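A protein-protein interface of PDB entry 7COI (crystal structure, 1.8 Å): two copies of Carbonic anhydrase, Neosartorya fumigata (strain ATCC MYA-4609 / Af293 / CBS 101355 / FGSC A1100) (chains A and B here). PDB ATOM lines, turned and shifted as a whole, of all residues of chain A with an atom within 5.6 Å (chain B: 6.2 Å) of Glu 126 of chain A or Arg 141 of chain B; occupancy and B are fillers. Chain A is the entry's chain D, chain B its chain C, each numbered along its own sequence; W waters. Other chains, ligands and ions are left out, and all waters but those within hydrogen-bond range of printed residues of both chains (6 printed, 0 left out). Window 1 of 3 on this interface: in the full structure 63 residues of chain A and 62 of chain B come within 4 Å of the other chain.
A ring nitrogen (ND1) of His 140 of chain A lies within hydrogen-bond range of the backbone carbonyl oxygen of Arg 141 of chain B, 2.8 Å away. The side-chain carboxylate (OE2) of Glu 126 of chain B lies within salt-bridge range of the guanidinium group (NH1) of Arg 141 of chain A, 3.2 Å away. ND1 of His 140 of chain B sits at hydrogen-bond distance from O of Arg 141 of chain A. The guanidinium group of Arg 141 of chain B lies within salt-bridge range of the side-chain carboxylate of Glu 126 of chain A. The guanidinium group of Arg 141 of chain B lies close to the side-chain hydroxyl of Thr 139 of chain A, at 3.4 Å. OG of Ser 120 of chain B lies within hydrogen-bond range of O of Thr 139 of chain A, 2.7 Å away. The guanidinium group (NH1) of Arg 141 of chain A lies within hydrogen-bond range of the side-chain hydroxyl (OG1) of Thr 139 of chain B, at 3.4 Å.
N of Ser 120 of chain B is in hydrogen-bond range of O of Asn 142 of chain B. The backbone NH of Asn 142 of chain B lies within hydrogen-bond range of the backbone carbonyl oxygen of Gly 118 of chain B (3.1 Å). The side-chain sulfur of Cys 119 of chain B lies close to the backbone NH of Asp 121 of chain B, 3.4 Å away. The side-chain carboxylate (OE1) of Glu 126 of chain A is in salt-bridge range of the guanidinium group (NH1) of Arg 141 of chain A (3.7 Å). The backbone carbonyl oxygen (O) of Cys 119 of chain B sits at hydrogen-bond distance from the guanidinium group (NE) of Arg 141 of chain B (3.0 Å). The side-chain sulfur of Cys 119 of chain B lies close to the backbone carbonyl oxygen of Asn 142 of chain B (3.6 Å).
CB of Pro 125 of chain A touches OE2 of Glu 126 of chain B, at 3.9 Å. Glu 126 of chain A touches Pro 125 of chain B (OE2 to CB, 3.8 Å). Thr 127 of chain A touches Pro 125 of chain B (OG1 to CB, 3.5 Å). Ser 122 of chain B touches Val 137 of chain A (CA to O, 3.3 Å). O of Ser 120 of chain B touches CD1 of Phe 138 of chain A, at 3.3 Å. N of Asp 121 of chain B touches CE1 of Phe 138 of chain A (3.6 Å). Phe 138 of chain A touches Ile 143 of chain B. Arg 141 of chain B touches Arg 141 of chain A (N to O, 3.7 Å). Ser 120 of chain B touches Val 157 of chain A (OG to CG2, 3.6 Å). Val 157 of chain A touches Ile 143 of chain B.
Printed residues of chain A within 4 Å of Ser 122 of chain B: Val 137 and Phe 138. Printed residues of chain A within 4 Å of Pro 125 of chain B: Glu 126 (3.8 Å) and Thr 127 (3.5 Å). Cys 119 of chain B touches none of the printed residues of chain A. The nearest residue of chain A that does not touch Arg 141 of chain B is Val 137 of chain A (4.2 Å).
Hydrophobic or aromatic side chains of chain A that line the printed part of chain B: Pro 125, Phe 138, His 140 and Val 157. Along chain B the printed residues that touch a printed residue of chain A span positions 120 to 143. Among the printed residues, 19 pairs touch across the chains.
Pro 125 of chain A touches Glu 126 of chain B, and with the chains exchanged Glu 126 of chain A touches Pro 125 of chain B. Glu 126 of chain A touches Arg 141 of chain B, and with the chains exchanged Arg 141 of chain A touches Glu 126 of chain B. Thr 139 of chain A touches Arg 141 of chain B, and with the chains exchanged Arg 141 of chain A touches Thr 139 of chain B. Arg 141 of chain B touches its own counterpart, Arg 141 of chain A. 7 positions are printed for both chains. Of the 19 pairs that touch across the chains among the printed residues, 9 have their exchanged pair printed and touching as well.
Water W6 lies within hydrogen-bond range of OE1 of Glu 126 of chain B, OE1 of Glu 126 of chain A, NH1 of Arg 141 of chain B and NH1 of Arg 141 of chain A. Water W2 lies within hydrogen-bond range of O of Val 137 of chain A (2.7 Å), NH2 of Arg 141 of chain B (2.9 Å) and O of Ser 122 of chain B (3.0 Å). Water W5 bridges the side-chain carboxylate of Glu 126 of chain B (2.7 Å) and the side-chain carboxylate of Glu 126 of chain A (2.9 Å). Water W3 lies within hydrogen-bond range of NE2 of His 140 of chain B (2.7 Å), OG of Ser 153 of chain A (2.8 Å) and ND2 of Asn 142 of chain B (2.9 Å). Water W1 bridges the backbone carbonyl oxygen of Ser 153 of chain A and the backbone NH of Ile 143 of chain B. Water W4 lies within hydrogen-bond range of the backbone NH (N) of Val 137 of chain A, the side-chain hydroxyl (OG1) of Thr 127 of chain A and the backbone carbonyl oxygen (O) of Ser 122 of chain B.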
ATOM      1  N   TRP A 116      13.375  13.455  17.869  1.00  0.00           N
ATOM      2  CA  TRP A 116      13.964  14.433  16.942  1.00  0.00           C
ATOM      3  C   TRP A 116      14.864  13.673  15.977  1.00  0.00           C
ATOM      4  O   TRP A 116      15.744  12.940  16.467  1.00  0.00           O
ATOM      5  CB  TRP A 116      14.809  15.424  17.737  1.00  0.00           C
ATOM      6  CG  TRP A 116      15.568  16.436  16.952  1.00  0.00           C
ATOM      7  CD1 TRP A 116      16.807  16.296  16.392  1.00  0.00           C
ATOM      8  CD2 TRP A 116      15.148  17.787  16.698  1.00  0.00           C
ATOM      9  NE1 TRP A 116      17.190  17.475  15.821  1.00  0.00           N
ATOM     10  CE2 TRP A 116      16.193  18.403  15.996  1.00  0.00           C
ATOM     11  CE3 TRP A 116      14.014  18.531  17.025  1.00  0.00           C
ATOM     12  CZ2 TRP A 116      16.141  19.733  15.607  1.00  0.00           C
ATOM     13  CZ3 TRP A 116      13.951  19.847  16.617  1.00  0.00           C
ATOM     14  CH2 TRP A 116      15.004  20.432  15.930  1.00  0.00           C
ATOM     15  N   CYS A 124      23.196  22.361  15.012  1.00  0.00           N
ATOM     16  CA  CYS A 124      21.783  21.944  15.238  1.00  0.00           C
ATOM     17  C   CYS A 124      21.654  21.016  16.440  1.00  0.00           C
ATOM     18  O   CYS A 124      21.024  19.960  16.341  1.00  0.00           O
ATOM     19  CB  CYS A 124      21.233  21.258  13.993  1.00  0.00           C
ATOM     20  SG  CYS A 124      21.546  22.171  12.480  1.00  0.00           S
ATOM     21  N   PRO A 125      22.163  21.371  17.657  1.00  0.00           N
ATOM     22  CA  PRO A 125      21.913  20.581  18.863  1.00  0.00           C
ATOM     23  C   PRO A 125      20.482  20.761  19.375  1.00  0.00           C
ATOM     24  O   PRO A 125      20.119  21.851  19.858  1.00  0.00           O
ATOM     25  CB  PRO A 125      22.918  21.101  19.894  1.00  0.00           C
ATOM     26  CG  PRO A 125      23.159  22.517  19.450  1.00  0.00           C
ATOM     27  CD  PRO A 125      23.025  22.523  17.947  1.00  0.00           C
ATOM     28  N   GLU A 126      19.687  19.698  19.278  1.00  0.00           N
ATOM     29  CA  GLU A 126      18.205  19.779  19.427  1.00  0.00           C
ATOM     30  C   GLU A 126      17.854  20.338  20.814  1.00  0.00           C
ATOM     31  O   GLU A 126      16.985  21.258  20.904  1.00  0.00           O
ATOM     32  CB  GLU A 126      17.554  18.418  19.162  1.00  0.00           C
ATOM     33  CG  GLU A 126      17.800  17.344  20.206  1.00  0.00           C
ATOM     34  CD  GLU A 126      19.251  17.052  20.508  1.00  0.00           C
ATOM     35  OE1 GLU A 126      20.021  16.941  19.539  1.00  0.00           O
ATOM     36  OE2 GLU A 126      19.621  17.033  21.724  1.00  0.00           O
ATOM     37  N   THR A 127      18.478  19.831  21.875  1.00  0.00           N
ATOM     38  CA  THR A 127      18.063  20.152  23.262  1.00  0.00           C
ATOM     39  C   THR A 127      18.351  21.634  23.502  1.00  0.00           C
ATOM     40  O   THR A 127      17.539  22.302  24.147  1.00  0.00           O
ATOM     41  CB  THR A 127      18.703  19.167  24.244  1.00  0.00           C
ATOM     42  OG1 THR A 127      18.216  17.869  23.893  1.00  0.00           O
ATOM     43  CG2 THR A 127      18.381  19.439  25.698  1.00  0.00           C
ATOM     44  N   THR A 128      19.476  22.135  23.011  1.00  0.00           N
ATOM     45  CA  THR A 128      19.873  23.542  23.178  1.00  0.00           C
ATOM     46  C   THR A 128      18.924  24.439  22.371  1.00  0.00           C
ATOM     47  O   THR A 128      18.413  25.420  22.946  1.00  0.00           O
ATOM     48  CB  THR A 128      21.312  23.751  22.720  1.00  0.00           C
ATOM     49  OG1 THR A 128      22.191  22.947  23.517  1.00  0.00           O
ATOM     50  CG2 THR A 128      21.710  25.206  22.798  1.00  0.00           C
ATOM     51  N   ILE A 129      18.696  24.155  21.086  1.00  0.00           N
ATOM     52  CA  ILE A 129      17.936  25.116  20.233  1.00  0.00           C
ATOM     53  C   ILE A 129      16.448  25.108  20.625  1.00  0.00           C
ATOM     54  O   ILE A 129      15.769  26.073  20.285  1.00  0.00           O
ATOM     55  CB  ILE A 129      18.161  24.880  18.733  1.00  0.00           C
ATOM     56  CG1 ILE A 129      17.486  23.602  18.237  1.00  0.00           C
ATOM     57  CG2 ILE A 129      19.662  24.931  18.391  1.00  0.00           C
ATOM     58  CD1 ILE A 129      17.727  23.378  16.741  1.00  0.00           C
ATOM     59  N   LEU A 130      15.979  24.073  21.299  1.00  0.00           N
ATOM     60  CA  LEU A 130      14.582  23.955  21.786  1.00  0.00           C
ATOM     61  C   LEU A 130      14.429  24.541  23.189  1.00  0.00           C
ATOM     62  O   LEU A 130      13.292  24.525  23.694  1.00  0.00           O
ATOM     63  CB  LEU A 130      14.145  22.490  21.746  1.00  0.00           C
ATOM     64  CG  LEU A 130      13.971  21.893  20.335  1.00  0.00           C
ATOM     65  CD1 LEU A 130      13.609  20.436  20.429  1.00  0.00           C
ATOM     66  CD2 LEU A 130      12.949  22.650  19.486  1.00  0.00           C
ATOM     67  N   GLY A 131      15.514  24.963  23.840  1.00  0.00           N
ATOM     68  CA  GLY A 131      15.473  25.422  25.245  1.00  0.00           C
ATOM     69  C   GLY A 131      14.982  24.353  26.196  1.00  0.00           C
ATOM     70  O   GLY A 131      14.275  24.687  27.151  1.00  0.00           O
ATOM     71  N   VAL A 137      14.228  15.017  24.884  1.00  0.00           N
ATOM     72  CA  VAL A 137      14.255  14.762  23.406  1.00  0.00           C
ATOM     73  C   VAL A 137      15.060  13.517  23.080  1.00  0.00           C
ATOM     74  O   VAL A 137      16.281  13.524  23.220  1.00  0.00           O
ATOM     75  CB  VAL A 137      14.755  15.977  22.612  1.00  0.00           C
ATOM     76  CG1 VAL A 137      14.564  15.757  21.114  1.00  0.00           C
ATOM     77  CG2 VAL A 137      14.048  17.269  23.014  1.00  0.00           C
ATOM     78  N   PHE A 138      14.370  12.458  22.644  1.00  0.00           N
ATOM     79  CA  PHE A 138      15.017  11.230  22.118  1.00  0.00           C
ATOM     80  C   PHE A 138      15.536  11.582  20.736  1.00  0.00           C
ATOM     81  O   PHE A 138      14.778  12.158  19.960  1.00  0.00           O
ATOM     82  CB  PHE A 138      14.046  10.061  22.154  1.00  0.00           C
ATOM     83  CG  PHE A 138      14.693   8.718  21.989  1.00  0.00           C
ATOM     84  CD1 PHE A 138      15.333   8.123  23.066  1.00  0.00           C
ATOM     85  CD2 PHE A 138      14.600   8.009  20.800  1.00  0.00           C
ATOM     86  CE1 PHE A 138      15.867   6.848  22.958  1.00  0.00           C
ATOM     87  CE2 PHE A 138      15.168   6.750  20.686  1.00  0.00           C
ATOM     88  CZ  PHE A 138      15.784   6.163  21.771  1.00  0.00           C
ATOM     89  N   THR A 139      16.808  11.336  20.450  1.00  0.00           N
ATOM     90  CA  THR A 139      17.493  12.007  19.323  1.00  0.00           C
ATOM     91  C   THR A 139      18.182  11.027  18.366  1.00  0.00           C
ATOM     92  O   THR A 139      18.967  10.203  18.804  1.00  0.00           O
ATOM     93  CB  THR A 139      18.487  13.057  19.829  1.00  0.00           C
ATOM     94  OG1 THR A 139      17.783  14.005  20.626  1.00  0.00           O
ATOM     95  CG2 THR A 139      19.188  13.751  18.686  1.00  0.00           C
ATOM     96  N   HIS A 140      17.961  11.247  17.066  1.00  0.00           N
ATOM     97  CA  HIS A 140      18.741  10.648  15.962  1.00  0.00           C
ATOM     98  C   HIS A 140      19.281  11.784  15.104  1.00  0.00           C
ATOM     99  O   HIS A 140      18.479  12.598  14.610  1.00  0.00           O
ATOM    100  CB  HIS A 140      17.897   9.652  15.165  1.00  0.00           C
ATOM    101  CG  HIS A 140      18.658   8.870  14.153  1.00  0.00           C
ATOM    102  ND1 HIS A 140      19.769   8.107  14.481  1.00  0.00           N
ATOM    103  CD2 HIS A 140      18.454   8.666  12.825  1.00  0.00           C
ATOM    104  CE1 HIS A 140      20.213   7.494  13.388  1.00  0.00           C
ATOM    105  NE2 HIS A 140      19.427   7.817  12.375  1.00  0.00           N
ATOM    106  N   ARG A 141      20.583  11.804  14.891  1.00  0.00           N
ATOM    107  CA  ARG A 141      21.234  12.795  13.999  1.00  0.00           C
ATOM    108  C   ARG A 141      22.141  12.047  13.026  1.00  0.00           C
ATOM    109  O   ARG A 141      22.906  11.167  13.481  1.00  0.00           O
ATOM    110  CB  ARG A 141      21.948  13.872  14.815  1.00  0.00           C
ATOM    111  CG  ARG A 141      20.960  14.831  15.469  1.00  0.00           C
ATOM    112  CD  ARG A 141      21.591  15.737  16.504  1.00  0.00           C
ATOM    113  NE  ARG A 141      22.477  16.725  15.932  1.00  0.00           N
ATOM    114  CZ  ARG A 141      23.291  17.493  16.651  1.00  0.00           C
ATOM    115  NH1 ARG A 141      23.345  17.395  17.966  1.00  0.00           N
ATOM    116  NH2 ARG A 141      24.032  18.384  16.053  1.00  0.00           N
ATOM    117  N   SER A 153      19.558   1.935  11.250  1.00  0.00           N
ATOM    118  CA  SER A 153      19.937   2.966  12.243  1.00  0.00           C
ATOM    119  C   SER A 153      18.716   3.834  12.597  1.00  0.00           C
ATOM    120  O   SER A 153      18.290   3.848  13.774  1.00  0.00           O
ATOM    121  CB  SER A 153      21.082   3.804  11.782  1.00  0.00           C
ATOM    122  OG  SER A 153      21.503   4.661  12.838  1.00  0.00           O
ATOM    123  N   VAL A 157      15.821   3.399  15.880  1.00  0.00           N
ATOM    124  CA  VAL A 157      15.454   4.588  16.688  1.00  0.00           C
ATOM    125  C   VAL A 157      13.931   4.767  16.679  1.00  0.00           C
ATOM    126  O   VAL A 157      13.329   4.991  17.768  1.00  0.00           O
ATOM    127  CB  VAL A 157      16.176   5.840  16.177  1.00  0.00           C
ATOM    128  CG1 VAL A 157      15.518   7.092  16.731  1.00  0.00           C
ATOM    129  CG2 VAL A 157      17.665   5.783  16.467  1.00  0.00           C
ATOM    130  N   TRP B 116      30.971  13.437  18.182  1.00  0.00           N
ATOM    131  CA  TRP B 116      30.369  12.664  19.276  1.00  0.00           C
ATOM    132  C   TRP B 116      29.513  11.559  18.661  1.00  0.00           C
ATOM    133  O   TRP B 116      28.658  11.888  17.837  1.00  0.00           O
ATOM    134  CB  TRP B 116      29.501  13.607  20.094  1.00  0.00           C
ATOM    135  CG  TRP B 116      28.744  12.980  21.214  1.00  0.00           C
ATOM    136  CD1 TRP B 116      27.519  12.402  21.149  1.00  0.00           C
ATOM    137  CD2 TRP B 116      29.120  12.990  22.599  1.00  0.00           C
ATOM    138  NE1 TRP B 116      27.097  12.062  22.399  1.00  0.00           N
ATOM    139  CE2 TRP B 116      28.070  12.398  23.306  1.00  0.00           C
ATOM    140  CE3 TRP B 116      30.253  13.427  23.300  1.00  0.00           C
ATOM    141  CZ2 TRP B 116      28.103  12.237  24.677  1.00  0.00           C
ATOM    142  CZ3 TRP B 116      30.264  13.282  24.664  1.00  0.00           C
ATOM    143  CH2 TRP B 116      29.208  12.697  25.344  1.00  0.00           C
ATOM    144  N   ILE B 117      29.757  10.315  19.048  1.00  0.00           N
ATOM    145  CA  ILE B 117      28.873   9.170  18.715  1.00  0.00           C
ATOM    146  C   ILE B 117      28.322   8.688  20.042  1.00  0.00           C
ATOM    147  O   ILE B 117      29.100   8.186  20.880  1.00  0.00           O
ATOM    148  CB  ILE B 117      29.583   8.067  17.913  1.00  0.00           C
ATOM    149  CG1 ILE B 117      30.237   8.609  16.634  1.00  0.00           C
ATOM    150  CG2 ILE B 117      28.586   6.956  17.636  1.00  0.00           C
ATOM    151  CD1 ILE B 117      31.185   7.659  15.948  1.00  0.00           C
ATOM    152  N   GLY B 118      27.040   8.914  20.263  1.00  0.00           N
ATOM    153  CA  GLY B 118      26.361   8.537  21.506  1.00  0.00           C
ATOM    154  C   GLY B 118      25.036   7.869  21.280  1.00  0.00           C
ATOM    155  O   GLY B 118      24.625   7.607  20.129  1.00  0.00           O
ATOM    156  N   CYS B 119      24.388   7.562  22.376  1.00  0.00           N
ATOM    157  CA  CYS B 119      23.048   6.943  22.384  1.00  0.00           C
ATOM    158  C   CYS B 119      21.996   8.022  22.115  1.00  0.00           C
ATOM    159  O   CYS B 119      22.149   9.182  22.555  1.00  0.00           O
ATOM    160  CB  CYS B 119      22.783   6.174  23.668  1.00  0.00           C
ATOM    161  SG  CYS B 119      21.303   5.236  23.464  1.00  0.00           S
ATOM    162  N   SER B 120      20.920   7.629  21.430  1.00  0.00           N
ATOM    163  CA  SER B 120      19.687   8.434  21.261  1.00  0.00           C
ATOM    164  C   SER B 120      18.995   8.750  22.585  1.00  0.00           C
ATOM    165  O   SER B 120      18.166   9.653  22.598  1.00  0.00           O
ATOM    166  CB  SER B 120      18.747   7.679  20.360  1.00  0.00           C
ATOM    167  OG  SER B 120      19.350   7.541  19.079  1.00  0.00           O
ATOM    168  N   ASP B 121      19.265   7.981  23.639  1.00  0.00           N
ATOM    169  CA  ASP B 121      18.709   8.200  24.997  1.00  0.00           C
ATOM    170  C   ASP B 121      18.580   9.711  25.255  1.00  0.00           C
ATOM    171  O   ASP B 121      19.572  10.458  25.075  1.00  0.00           O
ATOM    172  CB  ASP B 121      19.543   7.477  26.051  1.00  0.00           C
ATOM    173  CG  ASP B 121      18.863   7.413  27.402  1.00  0.00           C
ATOM    174  OD1 ASP B 121      18.564   8.481  27.952  1.00  0.00           O
ATOM    175  OD2 ASP B 121      18.578   6.289  27.857  1.00  0.00           O
ATOM    176  N   SER B 122      17.382  10.156  25.613  1.00  0.00           N
ATOM    177  CA  SER B 122      17.028  11.572  25.812  1.00  0.00           C
ATOM    178  C   SER B 122      17.876  12.175  26.949  1.00  0.00           C
ATOM    179  O   SER B 122      17.993  13.417  26.976  1.00  0.00           O
ATOM    180  CB  SER B 122      15.583  11.726  26.119  1.00  0.00           C
ATOM    181  OG  SER B 122      15.243  11.125  27.372  1.00  0.00           O
ATOM    182  N   ARG B 123      18.484  11.347  27.781  1.00  0.00           N
ATOM    183  CA  ARG B 123      19.279  11.860  28.930  1.00  0.00           C
ATOM    184  C   ARG B 123      20.701  12.212  28.510  1.00  0.00           C
ATOM    185  O   ARG B 123      21.417  12.704  29.384  1.00  0.00           O
ATOM    186  CB  ARG B 123      19.240  10.844  30.061  1.00  0.00           C
ATOM    187  CG  ARG B 123      17.836  10.586  30.557  1.00  0.00           C
ATOM    188  CD  ARG B 123      17.772   9.382  31.487  1.00  0.00           C
ATOM    189  NE  ARG B 123      17.971   8.142  30.766  1.00  0.00           N
ATOM    190  CZ  ARG B 123      17.858   6.920  31.295  1.00  0.00           C
ATOM    191  NH1 ARG B 123      17.533   6.753  32.573  1.00  0.00           N
ATOM    192  NH2 ARG B 123      18.048   5.859  30.534  1.00  0.00           N
ATOM    193  N   CYS B 124      21.099  12.009  27.245  1.00  0.00           N
ATOM    194  CA  CYS B 124      22.503  12.182  26.791  1.00  0.00           C
ATOM    195  C   CYS B 124      22.608  13.218  25.671  1.00  0.00           C
ATOM    196  O   CYS B 124      23.234  12.961  24.654  1.00  0.00           O
ATOM    197  CB  CYS B 124      23.072  10.824  26.370  1.00  0.00           C
ATOM    198  SG  CYS B 124      22.708   9.467  27.539  1.00  0.00           S
ATOM    199  N   PRO B 125      22.069  14.459  25.816  1.00  0.00           N
ATOM    200  CA  PRO B 125      22.317  15.531  24.840  1.00  0.00           C
ATOM    201  C   PRO B 125      23.736  16.101  24.943  1.00  0.00           C
ATOM    202  O   PRO B 125      24.060  16.794  25.934  1.00  0.00           O
ATOM    203  CB  PRO B 125      21.281  16.616  25.160  1.00  0.00           C
ATOM    204  CG  PRO B 125      21.042  16.405  26.628  1.00  0.00           C
ATOM    205  CD  PRO B 125      21.162  14.913  26.869  1.00  0.00           C
ATOM    206  N   GLU B 126      24.553  15.829  23.931  1.00  0.00           N
ATOM    207  CA  GLU B 126      26.026  15.996  24.011  1.00  0.00           C
ATOM    208  C   GLU B 126      26.374  17.461  24.338  1.00  0.00           C
ATOM    209  O   GLU B 126      27.229  17.706  25.238  1.00  0.00           O
ATOM    210  CB  GLU B 126      26.724  15.506  22.740  1.00  0.00           C
ATOM    211  CG  GLU B 126      26.494  16.341  21.496  1.00  0.00           C
ATOM    212  CD  GLU B 126      25.038  16.568  21.123  1.00  0.00           C
ATOM    213  OE1 GLU B 126      24.271  15.559  21.178  1.00  0.00           O
ATOM    214  OE2 GLU B 126      24.651  17.745  20.886  1.00  0.00           O
ATOM    215  N   THR B 139      27.562  15.567  15.553  1.00  0.00           N
ATOM    216  CA  THR B 139      26.894  14.552  16.409  1.00  0.00           C
ATOM    217  C   THR B 139      26.213  13.438  15.597  1.00  0.00           C
ATOM    218  O   THR B 139      25.476  13.736  14.683  1.00  0.00           O
ATOM    219  CB  THR B 139      25.867  15.206  17.329  1.00  0.00           C
ATOM    220  OG1 THR B 139      26.517  16.201  18.117  1.00  0.00           O
ATOM    221  CG2 THR B 139      25.181  14.197  18.206  1.00  0.00           C
ATOM    222  N   HIS B 140      26.476  12.198  15.997  1.00  0.00           N
ATOM    223  CA  HIS B 140      25.692  10.998  15.622  1.00  0.00           C
ATOM    224  C   HIS B 140      25.159  10.334  16.873  1.00  0.00           C
ATOM    225  O   HIS B 140      25.942  10.017  17.794  1.00  0.00           O
ATOM    226  CB  HIS B 140      26.565  10.054  14.789  1.00  0.00           C
ATOM    227  CG  HIS B 140      25.823   8.932  14.151  1.00  0.00           C
ATOM    228  ND1 HIS B 140      24.737   9.144  13.340  1.00  0.00           N
ATOM    229  CD2 HIS B 140      26.021   7.594  14.166  1.00  0.00           C
ATOM    230  CE1 HIS B 140      24.317   7.980  12.858  1.00  0.00           C
ATOM    231  NE2 HIS B 140      25.061   7.013  13.368  1.00  0.00           N
ATOM    232  N   ARG B 141      23.852  10.108  16.919  1.00  0.00           N
ATOM    233  CA  ARG B 141      23.217   9.388  18.037  1.00  0.00           C
ATOM    234  C   ARG B 141      22.327   8.294  17.456  1.00  0.00           C
ATOM    235  O   ARG B 141      21.554   8.593  16.520  1.00  0.00           O
ATOM    236  CB  ARG B 141      22.457  10.346  18.947  1.00  0.00           C
ATOM    237  CG  ARG B 141      23.394  11.206  19.792  1.00  0.00           C
ATOM    238  CD  ARG B 141      22.676  12.361  20.417  1.00  0.00           C
ATOM    239  NE  ARG B 141      21.797  11.961  21.485  1.00  0.00           N
ATOM    240  CZ  ARG B 141      21.005  12.788  22.157  1.00  0.00           C
ATOM    241  NH1 ARG B 141      20.948  14.069  21.852  1.00  0.00           N
ATOM    242  NH2 ARG B 141      20.253  12.322  23.124  1.00  0.00           N
ATOM    243  N   ASN B 142      22.479   7.075  17.986  1.00  0.00           N
ATOM    244  CA  ASN B 142      21.739   5.886  17.504  1.00  0.00           C
ATOM    245  C   ASN B 142      21.407   5.042  18.723  1.00  0.00           C
ATOM    246  O   ASN B 142      21.770   5.405  19.870  1.00  0.00           O
ATOM    247  CB  ASN B 142      22.506   5.180  16.379  1.00  0.00           C
ATOM    248  CG  ASN B 142      23.772   4.503  16.854  1.00  0.00           C
ATOM    249  OD1 ASN B 142      23.893   4.243  18.058  1.00  0.00           O
ATOM    250  ND2 ASN B 142      24.666   4.203  15.924  1.00  0.00           N
ATOM    251  N   ILE B 143      20.723   3.928  18.517  1.00  0.00           N
ATOM    252  CA  ILE B 143      20.393   3.020  19.649  1.00  0.00           C
ATOM    253  C   ILE B 143      21.672   2.384  20.205  1.00  0.00           C
ATOM    254  O   ILE B 143      22.335   1.621  19.503  1.00  0.00           O
ATOM    255  CB  ILE B 143      19.335   1.976  19.262  1.00  0.00           C
ATOM    256  CG1 ILE B 143      18.038   2.683  18.872  1.00  0.00           C
ATOM    257  CG2 ILE B 143      19.182   0.987  20.430  1.00  0.00           C
ATOM    258  CD1 ILE B 143      17.405   3.487  19.959  1.00  0.00           C
HETATM  259  O   HOH W   1      19.934   2.932  15.858  1.00  0.00           O
HETATM  260  O   HOH W   2      18.584  14.385  24.222  1.00  0.00           O
HETATM  261  O   HOH W   3      24.239   4.408  13.109  1.00  0.00           O
HETATM  262  O   HOH W   4      16.671  16.241  25.825  1.00  0.00           O
HETATM  263  O   HOH W   5      22.246  18.185  22.096  1.00  0.00           O
HETATM  264  O   HOH W   6      22.140  15.513  19.771  1.00  0.00           O
